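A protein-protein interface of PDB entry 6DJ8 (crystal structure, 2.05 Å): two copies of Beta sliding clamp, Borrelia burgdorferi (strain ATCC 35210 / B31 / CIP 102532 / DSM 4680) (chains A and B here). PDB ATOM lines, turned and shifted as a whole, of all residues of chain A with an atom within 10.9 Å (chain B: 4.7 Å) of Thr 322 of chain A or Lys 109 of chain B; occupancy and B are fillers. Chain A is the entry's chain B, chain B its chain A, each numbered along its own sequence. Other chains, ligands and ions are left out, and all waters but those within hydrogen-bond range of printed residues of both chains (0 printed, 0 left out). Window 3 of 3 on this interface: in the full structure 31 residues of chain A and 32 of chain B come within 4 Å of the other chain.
The side-chain amino group (NZ) of Lys 109 of chain B sits at hydrogen-bond distance from the backbone carbonyl oxygen (O) of Thr 322 of chain A (3.2 Å). The backbone NH of Lys 128 of chain B sits at hydrogen-bond distance from the backbone carbonyl oxygen of Lys 325 of chain A. OE2 of Glu 129 of chain B sits at hydrogen-bond distance from OH of Tyr 297 of chain A. The side-chain carboxylate of Glu 129 of chain B is in salt-bridge range of the guanidinium group of Arg 324 of chain A.
Gly 323 of chain A touches Lys 109 of chain B (O to CE, 3.7 Å). O of Lys 128 of chain B touches CA of Arg 324 of chain A, 3.4 Å away. Arg 324 of chain A touches Pro 130 of chain B.
Printed residues of chain B within 4 Å of Tyr 297 of chain A: Glu 129. Glu 318 of chain A touches none of the printed residues of chain B. Leu 320 of chain A touches none of the printed residues of chain B. Thr 322 of chain A touches one residue of chain B. Of the printed residues of chain B, Gly 323 of chain A touches Lys 109. Of the printed residues of chain B, Lys 325 of chain A touches Lys 128. No residue of chain A comes within 4 Å of Asn 104 of chain B. No residue of chain A comes within 4 Å of Asn 107 of chain B. No residue of chain A comes within 4 Å of Ser 108 of chain B. Printed residues of chain A within 4 Å of Lys 109 of chain B: Thr 322 and Gly 323. No residue of chain A comes within 4 Å of Glu 111 of chain B. Printed residues of chain A within 4 Å of Glu 129 of chain B: Tyr 297 and Arg 324. No residue of chain A comes within 4 Å of Thr 131 of chain B. The nearest residue of chain B that does not touch Thr 322 of chain A is Met 38 of chain B (4.04 Å). The nearest printed residue of chain A that does not touch Lys 128 of chain B is Gly 323 of chain A (4.01 Å).
No position is printed for both chains. Of the 7 pairs that touch across the chains among the printed residues, none has its exchanged pair printed and touching as well.
Of the 13 printed residues of chain B, 4 touch a printed residue of chain A. Hydrophobic or aromatic side chains of chain B within 4 Å of the printed part of chain A: Pro 130. Of the 14 printed residues of chain A, 5 touch a printed residue of chain B. Hydrophobic or aromatic side chains of chain A that line the printed part of chain B: Tyr 297. Among the printed residues, 7 pairs touch across the chains. Among the printed residues, Asp or Glu carboxylates within 4 Å of a Lys or Arg side-chain nitrogen of the other chain: Arg 324 of chain A with Glu 129 of chain B (2.8 Å).
The backbone NH (N) of Asn 104 of chain B lies within hydrogen-bond range of the backbone carbonyl oxygen (O) of Lys 109 of chain B, 2.7 Å away. The backbone NH of Lys 109 of chain B lies within hydrogen-bond range of the side-chain hydroxyl of Thr 131 of chain B, at 3.5 Å. O of Glu 129 of chain B sits at hydrogen-bond distance from N of Leu 110 of chain B (2.7 Å). The backbone NH of Glu 318 of chain A sits at hydrogen-bond distance from the backbone carbonyl oxygen of Tyr 297 of chain A. The side-chain carboxylate (OD1) of Asp 319 of chain A sits at hydrogen-bond distance from the backbone NH (N) of Thr 322 of chain A. The backbone NH of Arg 324 of chain A is in hydrogen-bond range of the side-chain hydroxyl of Thr 322 of chain A.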
ATOM      1  N   LEU A 296     -20.526   6.292 -20.939  1.00  0.00           N
ATOM      2  CA  LEU A 296     -19.931   5.249 -21.782  1.00  0.00           C
ATOM      3  C   LEU A 296     -18.449   5.483 -22.023  1.00  0.00           C
ATOM      4  O   LEU A 296     -17.815   4.666 -22.707  1.00  0.00           O
ATOM      5  CB  LEU A 296     -20.675   5.177 -23.123  1.00  0.00           C
ATOM      6  CG  LEU A 296     -22.153   4.756 -23.046  1.00  0.00           C
ATOM      7  CD1 LEU A 296     -22.866   4.996 -24.375  1.00  0.00           C
ATOM      8  CD2 LEU A 296     -22.309   3.308 -22.606  1.00  0.00           C
ATOM      9  N   TYR A 297     -17.909   6.618 -21.542  1.00  0.00           N
ATOM     10  CA  TYR A 297     -16.504   6.977 -21.697  1.00  0.00           C
ATOM     11  C   TYR A 297     -15.805   7.183 -20.355  1.00  0.00           C
ATOM     12  O   TYR A 297     -14.669   7.692 -20.326  1.00  0.00           O
ATOM     13  CB  TYR A 297     -16.370   8.238 -22.576  1.00  0.00           C
ATOM     14  CG  TYR A 297     -16.730   7.940 -24.022  1.00  0.00           C
ATOM     15  CD1 TYR A 297     -18.053   8.002 -24.459  1.00  0.00           C
ATOM     16  CD2 TYR A 297     -15.754   7.551 -24.933  1.00  0.00           C
ATOM     17  CE1 TYR A 297     -18.395   7.685 -25.777  1.00  0.00           C
ATOM     18  CE2 TYR A 297     -16.083   7.232 -26.246  1.00  0.00           C
ATOM     19  CZ  TYR A 297     -17.395   7.305 -26.658  1.00  0.00           C
ATOM     20  OH  TYR A 297     -17.701   7.014 -27.956  1.00  0.00           O
ATOM     21  N   VAL A 298     -16.442   6.778 -19.253  1.00  0.00           N
ATOM     22  CA  VAL A 298     -15.891   6.896 -17.902  1.00  0.00           C
ATOM     23  C   VAL A 298     -15.469   5.504 -17.446  1.00  0.00           C
ATOM     24  O   VAL A 298     -16.228   4.541 -17.606  1.00  0.00           O
ATOM     25  CB  VAL A 298     -16.930   7.492 -16.939  1.00  0.00           C
ATOM     26  CG1 VAL A 298     -16.369   7.578 -15.537  1.00  0.00           C
ATOM     27  CG2 VAL A 298     -17.392   8.848 -17.431  1.00  0.00           C
ATOM     28  N   ASP A 299     -14.270   5.387 -16.888  1.00  0.00           N
ATOM     29  CA  ASP A 299     -13.753   4.063 -16.563  1.00  0.00           C
ATOM     30  C   ASP A 299     -14.221   3.635 -15.172  1.00  0.00           C
ATOM     31  O   ASP A 299     -15.095   4.258 -14.558  1.00  0.00           O
ATOM     32  CB  ASP A 299     -12.230   4.032 -16.681  1.00  0.00           C
ATOM     33  CG  ASP A 299     -11.531   4.910 -15.647  1.00  0.00           C
ATOM     34  OD1 ASP A 299     -12.171   5.370 -14.675  1.00  0.00           O
ATOM     35  OD2 ASP A 299     -10.320   5.148 -15.823  1.00  0.00           O
ATOM     36  N   GLY A 317     -15.365  12.386 -20.462  1.00  0.00           N
ATOM     37  CA  GLY A 317     -14.977  11.048 -20.057  1.00  0.00           C
ATOM     38  C   GLY A 317     -13.757  10.642 -20.843  1.00  0.00           C
ATOM     39  O   GLY A 317     -13.808  10.581 -22.080  1.00  0.00           O
ATOM     40  N   GLU A 318     -12.647  10.379 -20.163  1.00  0.00           N
ATOM     41  CA  GLU A 318     -11.405  10.129 -20.879  1.00  0.00           C
ATOM     42  C   GLU A 318     -10.647   8.994 -20.218  1.00  0.00           C
ATOM     43  O   GLU A 318     -10.647   8.869 -18.991  1.00  0.00           O
ATOM     44  CB  GLU A 318     -10.524  11.388 -20.951  1.00  0.00           C
ATOM     45  CG  GLU A 318      -9.275  11.211 -21.817  1.00  0.00           C
ATOM     46  CD  GLU A 318      -8.488  12.496 -22.024  1.00  0.00           C
ATOM     47  OE1 GLU A 318      -8.467  13.344 -21.106  1.00  0.00           O
ATOM     48  OE2 GLU A 318      -7.880  12.653 -23.108  1.00  0.00           O
ATOM     49  N   ASP A 319     -10.046   8.141 -21.042  1.00  0.00           N
ATOM     50  CA  ASP A 319      -9.147   7.092 -20.584  1.00  0.00           C
ATOM     51  C   ASP A 319      -7.773   7.489 -21.101  1.00  0.00           C
ATOM     52  O   ASP A 319      -7.517   7.415 -22.307  1.00  0.00           O
ATOM     53  CB  ASP A 319      -9.598   5.724 -21.094  1.00  0.00           C
ATOM     54  CG  ASP A 319      -8.743   4.583 -20.570  1.00  0.00           C
ATOM     55  OD1 ASP A 319      -7.509   4.601 -20.776  1.00  0.00           O
ATOM     56  OD2 ASP A 319      -9.321   3.672 -19.930  1.00  0.00           O
ATOM     57  N   LEU A 320      -6.896   7.928 -20.196  1.00  0.00           N
ATOM     58  CA  LEU A 320      -5.634   8.516 -20.636  1.00  0.00           C
ATOM     59  C   LEU A 320      -4.708   7.489 -21.271  1.00  0.00           C
ATOM     60  O   LEU A 320      -3.910   7.842 -22.148  1.00  0.00           O
ATOM     61  CB  LEU A 320      -4.928   9.213 -19.477  1.00  0.00           C
ATOM     62  CG  LEU A 320      -4.249  10.491 -19.975  1.00  0.00           C
ATOM     63  CD1 LEU A 320      -5.280  11.611 -20.072  1.00  0.00           C
ATOM     64  CD2 LEU A 320      -3.045  10.894 -19.121  1.00  0.00           C
ATOM     65  N   ILE A 321      -4.782   6.230 -20.835  1.00  0.00           N
ATOM     66  CA  ILE A 321      -3.917   5.197 -21.401  1.00  0.00           C
ATOM     67  C   ILE A 321      -4.221   5.000 -22.883  1.00  0.00           C
ATOM     68  O   ILE A 321      -3.325   5.059 -23.733  1.00  0.00           O
ATOM     69  CB  ILE A 321      -4.074   3.883 -20.616  1.00  0.00           C
ATOM     70  N   THR A 322      -5.498   4.792 -23.216  1.00  0.00           N
ATOM     71  CA  THR A 322      -5.889   4.431 -24.577  1.00  0.00           C
ATOM     72  C   THR A 322      -6.151   5.631 -25.478  1.00  0.00           C
ATOM     73  O   THR A 322      -5.996   5.521 -26.696  1.00  0.00           O
ATOM     74  CB  THR A 322      -7.127   3.519 -24.554  1.00  0.00           C
ATOM     75  OG1 THR A 322      -8.275   4.240 -24.076  1.00  0.00           O
ATOM     76  CG2 THR A 322      -6.889   2.297 -23.681  1.00  0.00           C
ATOM     77  N   GLY A 323      -6.557   6.770 -24.928  1.00  0.00           N
ATOM     78  CA  GLY A 323      -6.975   7.889 -25.741  1.00  0.00           C
ATOM     79  C   GLY A 323      -8.456   7.917 -26.054  1.00  0.00           C
ATOM     80  O   GLY A 323      -8.934   8.902 -26.636  1.00  0.00           O
ATOM     81  N   ARG A 324      -9.198   6.881 -25.670  1.00  0.00           N
ATOM     82  CA  ARG A 324     -10.643   6.886 -25.851  1.00  0.00           C
ATOM     83  C   ARG A 324     -11.266   8.022 -25.055  1.00  0.00           C
ATOM     84  O   ARG A 324     -11.053   8.130 -23.842  1.00  0.00           O
ATOM     85  CB  ARG A 324     -11.231   5.557 -25.397  1.00  0.00           C
ATOM     86  CG  ARG A 324     -12.656   5.388 -25.800  1.00  0.00           C
ATOM     87  CD  ARG A 324     -13.062   3.930 -25.725  1.00  0.00           C
ATOM     88  NE  ARG A 324     -14.424   3.793 -26.189  1.00  0.00           N
ATOM     89  CZ  ARG A 324     -15.491   3.804 -25.407  1.00  0.00           C
ATOM     90  NH1 ARG A 324     -16.686   3.683 -25.960  1.00  0.00           N
ATOM     91  NH2 ARG A 324     -15.369   3.929 -24.084  1.00  0.00           N
ATOM     92  N   LYS A 325     -12.093   8.828 -25.721  1.00  0.00           N
ATOM     93  CA  LYS A 325     -12.540  10.074 -25.108  1.00  0.00           C
ATOM     94  C   LYS A 325     -13.932  10.442 -25.606  1.00  0.00           C
ATOM     95  O   LYS A 325     -14.243  10.288 -26.789  1.00  0.00           O
ATOM     96  CB  LYS A 325     -11.515  11.175 -25.431  1.00  0.00           C
ATOM     97  CG  LYS A 325     -11.853  12.586 -25.014  1.00  0.00           C
ATOM     98  CD  LYS A 325     -10.609  13.468 -25.120  1.00  0.00           C
ATOM     99  CE  LYS A 325     -10.768  14.565 -26.153  1.00  0.00           C
ATOM    100  NZ  LYS A 325      -9.793  15.699 -25.916  1.00  0.00           N
ATOM    101  N   GLY A 326     -14.772  10.906 -24.692  1.00  0.00           N
ATOM    102  CA  GLY A 326     -16.066  11.452 -25.069  1.00  0.00           C
ATOM    103  C   GLY A 326     -16.305  12.802 -24.414  1.00  0.00           C
ATOM    104  O   GLY A 326     -16.187  12.928 -23.193  1.00  0.00           O
ATOM    105  N   MET B  38     -10.536  -5.110 -25.500  1.00  0.00           N
ATOM    106  CA  MET B  38     -10.454  -4.065 -26.510  1.00  0.00           C
ATOM    107  C   MET B  38      -9.237  -4.201 -27.420  1.00  0.00           C
ATOM    108  O   MET B  38      -9.281  -3.733 -28.564  1.00  0.00           O
ATOM    109  CB  MET B  38     -10.446  -2.723 -25.777  1.00  0.00           C
ATOM    110  CG  MET B  38     -10.062  -1.509 -26.565  1.00  0.00           C
ATOM    111  SD  MET B  38     -10.011  -0.116 -25.416  1.00  0.00           S
ATOM    112  CE  MET B  38      -9.795   1.231 -26.552  1.00  0.00           C
ATOM    113  N   VAL B 102     -14.797  10.201 -38.907  1.00  0.00           N
ATOM    114  CA  VAL B 102     -13.534  10.591 -39.516  1.00  0.00           C
ATOM    115  C   VAL B 102     -12.487   9.586 -39.072  1.00  0.00           C
ATOM    116  O   VAL B 102     -12.406   9.260 -37.885  1.00  0.00           O
ATOM    117  CB  VAL B 102     -13.124  12.019 -39.106  1.00  0.00           C
ATOM    118  CG1 VAL B 102     -11.776  12.385 -39.726  1.00  0.00           C
ATOM    119  CG2 VAL B 102     -14.191  13.021 -39.505  1.00  0.00           C
ATOM    120  N   PHE B 103     -11.704   9.078 -40.014  1.00  0.00           N
ATOM    121  CA  PHE B 103     -10.642   8.146 -39.668  1.00  0.00           C
ATOM    122  C   PHE B 103      -9.341   8.925 -39.611  1.00  0.00           C
ATOM    123  O   PHE B 103      -8.917   9.508 -40.613  1.00  0.00           O
ATOM    124  CB  PHE B 103     -10.544   6.982 -40.653  1.00  0.00           C
ATOM    125  CG  PHE B 103      -9.421   6.027 -40.348  1.00  0.00           C
ATOM    126  CD1 PHE B 103      -9.135   5.674 -39.041  1.00  0.00           C
ATOM    127  CD2 PHE B 103      -8.694   5.432 -41.365  1.00  0.00           C
ATOM    128  CE1 PHE B 103      -8.121   4.790 -38.745  1.00  0.00           C
ATOM    129  CE2 PHE B 103      -7.677   4.538 -41.078  1.00  0.00           C
ATOM    130  CZ  PHE B 103      -7.391   4.214 -39.767  1.00  0.00           C
ATOM    131  N   ASN B 104      -8.694   8.881 -38.457  1.00  0.00           N
ATOM    132  CA  ASN B 104      -7.428   9.565 -38.199  1.00  0.00           C
ATOM    133  C   ASN B 104      -6.394   8.455 -38.182  1.00  0.00           C
ATOM    134  O   ASN B 104      -6.082   7.890 -37.132  1.00  0.00           O
ATOM    135  CB  ASN B 104      -7.490  10.312 -36.861  1.00  0.00           C
ATOM    136  CG  ASN B 104      -6.245  11.145 -36.575  1.00  0.00           C
ATOM    137  OD1 ASN B 104      -6.138  11.753 -35.505  1.00  0.00           O
ATOM    138  ND2 ASN B 104      -5.311  11.181 -37.512  1.00  0.00           N
ATOM    139  N   ASN B 107      -3.251   8.748 -35.904  1.00  0.00           N
ATOM    140  CA  ASN B 107      -3.368   8.489 -34.479  1.00  0.00           C
ATOM    141  C   ASN B 107      -4.114   7.196 -34.165  1.00  0.00           C
ATOM    142  O   ASN B 107      -4.368   6.912 -32.988  1.00  0.00           O
ATOM    143  CB  ASN B 107      -4.054   9.677 -33.784  1.00  0.00           C
ATOM    144  CG  ASN B 107      -3.152  10.908 -33.704  1.00  0.00           C
ATOM    145  OD1 ASN B 107      -1.926  10.792 -33.659  1.00  0.00           O
ATOM    146  ND2 ASN B 107      -3.761  12.092 -33.699  1.00  0.00           N
ATOM    147  N   SER B 108      -4.482   6.417 -35.177  1.00  0.00           N
ATOM    148  CA  SER B 108      -5.273   5.200 -34.999  1.00  0.00           C
ATOM    149  C   SER B 108      -6.527   5.479 -34.171  1.00  0.00           C
ATOM    150  O   SER B 108      -6.765   4.887 -33.122  1.00  0.00           O
ATOM    151  CB  SER B 108      -4.427   4.094 -34.370  1.00  0.00           C
ATOM    152  OG  SER B 108      -3.465   3.611 -35.296  1.00  0.00           O
ATOM    153  N   LYS B 109      -7.326   6.415 -34.676  1.00  0.00           N
ATOM    154  CA  LYS B 109      -8.525   6.865 -33.992  1.00  0.00           C
ATOM    155  C   LYS B 109      -9.615   7.177 -35.003  1.00  0.00           C
ATOM    156  O   LYS B 109      -9.346   7.636 -36.117  1.00  0.00           O
ATOM    157  CB  LYS B 109      -8.261   8.103 -33.124  1.00  0.00           C
ATOM    158  CG  LYS B 109      -8.044   7.770 -31.658  1.00  0.00           C
ATOM    159  CD  LYS B 109      -7.069   8.727 -31.014  1.00  0.00           C
ATOM    160  CE  LYS B 109      -6.747   8.321 -29.575  1.00  0.00           C
ATOM    161  NZ  LYS B 109      -6.019   7.019 -29.495  1.00  0.00           N
ATOM    162  N   LEU B 110     -10.835   6.883 -34.605  1.00  0.00           N
ATOM    163  CA  LEU B 110     -12.030   7.357 -35.272  1.00  0.00           C
ATOM    164  C   LEU B 110     -12.496   8.584 -34.498  1.00  0.00           C
ATOM    165  O   LEU B 110     -12.581   8.541 -33.270  1.00  0.00           O
ATOM    166  CB  LEU B 110     -13.093   6.267 -35.264  1.00  0.00           C
ATOM    167  CG  LEU B 110     -13.572   5.728 -36.606  1.00  0.00           C
ATOM    168  CD1 LEU B 110     -12.410   5.182 -37.371  1.00  0.00           C
ATOM    169  CD2 LEU B 110     -14.582   4.621 -36.329  1.00  0.00           C
ATOM    170  N   GLU B 111     -12.717   9.688 -35.196  1.00  0.00           N
ATOM    171  CA  GLU B 111     -13.222  10.903 -34.578  1.00  0.00           C
ATOM    172  C   GLU B 111     -14.646  11.043 -35.078  1.00  0.00           C
ATOM    173  O   GLU B 111     -14.884  11.046 -36.292  1.00  0.00           O
ATOM    174  CB  GLU B 111     -12.378  12.116 -34.960  1.00  0.00           C
ATOM    175  CG  GLU B 111     -10.881  11.826 -34.968  1.00  0.00           C
ATOM    176  CD  GLU B 111     -10.132  12.556 -33.877  1.00  0.00           C
ATOM    177  OE1 GLU B 111     -10.776  13.276 -33.084  1.00  0.00           O
ATOM    178  OE2 GLU B 111      -8.893  12.413 -33.814  1.00  0.00           O
ATOM    179  N   LYS B 128     -13.757  10.092 -29.498  1.00  0.00           N
ATOM    180  CA  LYS B 128     -12.533   9.567 -30.092  1.00  0.00           C
ATOM    181  C   LYS B 128     -12.464   8.088 -29.765  1.00  0.00           C
ATOM    182  O   LYS B 128     -12.392   7.718 -28.588  1.00  0.00           O
ATOM    183  CB  LYS B 128     -11.281  10.292 -29.576  1.00  0.00           C
ATOM    184  CG  LYS B 128     -11.194  11.746 -29.981  1.00  0.00           C
ATOM    185  CD  LYS B 128      -9.810  12.333 -29.669  1.00  0.00           C
ATOM    186  CE  LYS B 128      -9.725  13.797 -30.084  1.00  0.00           C
ATOM    187  NZ  LYS B 128      -8.469  14.479 -29.603  1.00  0.00           N
ATOM    188  N   GLU B 129     -12.478   7.253 -30.803  1.00  0.00           N
ATOM    189  CA  GLU B 129     -12.468   5.800 -30.643  1.00  0.00           C
ATOM    190  C   GLU B 129     -11.184   5.232 -31.229  1.00  0.00           C
ATOM    191  O   GLU B 129     -10.971   5.306 -32.456  1.00  0.00           O
ATOM    192  CB  GLU B 129     -13.683   5.173 -31.320  1.00  0.00           C
ATOM    193  CG  GLU B 129     -15.017   5.479 -30.630  1.00  0.00           C
ATOM    194  CD  GLU B 129     -15.170   4.756 -29.286  1.00  0.00           C
ATOM    195  OE1 GLU B 129     -14.319   3.896 -28.952  1.00  0.00           O
ATOM    196  OE2 GLU B 129     -16.162   5.041 -28.566  1.00  0.00           O
ATOM    197  N   PRO B 130     -10.312   4.668 -30.409  1.00  0.00           N
ATOM    198  CA  PRO B 130      -9.081   4.084 -30.939  1.00  0.00           C
ATOM    199  C   PRO B 130      -9.385   2.892 -31.825  1.00  0.00           C
ATOM    200  O   PRO B 130     -10.386   2.193 -31.645  1.00  0.00           O
ATOM    201  CB  PRO B 130      -8.277   3.686 -29.692  1.00  0.00           C
ATOM    202  CG  PRO B 130      -9.226   3.832 -28.522  1.00  0.00           C
ATOM    203  CD  PRO B 130     -10.203   4.891 -28.962  1.00  0.00           C
ATOM    204  N   THR B 131      -8.528   2.708 -32.822  1.00  0.00           N
ATOM    205  CA  THR B 131      -8.673   1.661 -33.827  1.00  0.00           C
ATOM    206  C   THR B 131      -7.431   0.789 -33.870  1.00  0.00           C
ATOM    207  O   THR B 131      -6.399   1.103 -33.275  1.00  0.00           O
ATOM    208  CB  THR B 131      -8.925   2.261 -35.215  1.00  0.00           C
ATOM    209  OG1 THR B 131      -7.798   3.080 -35.575  1.00  0.00           O
ATOM    210  CG2 THR B 131     -10.186   3.103 -35.212  1.00  0.00           C
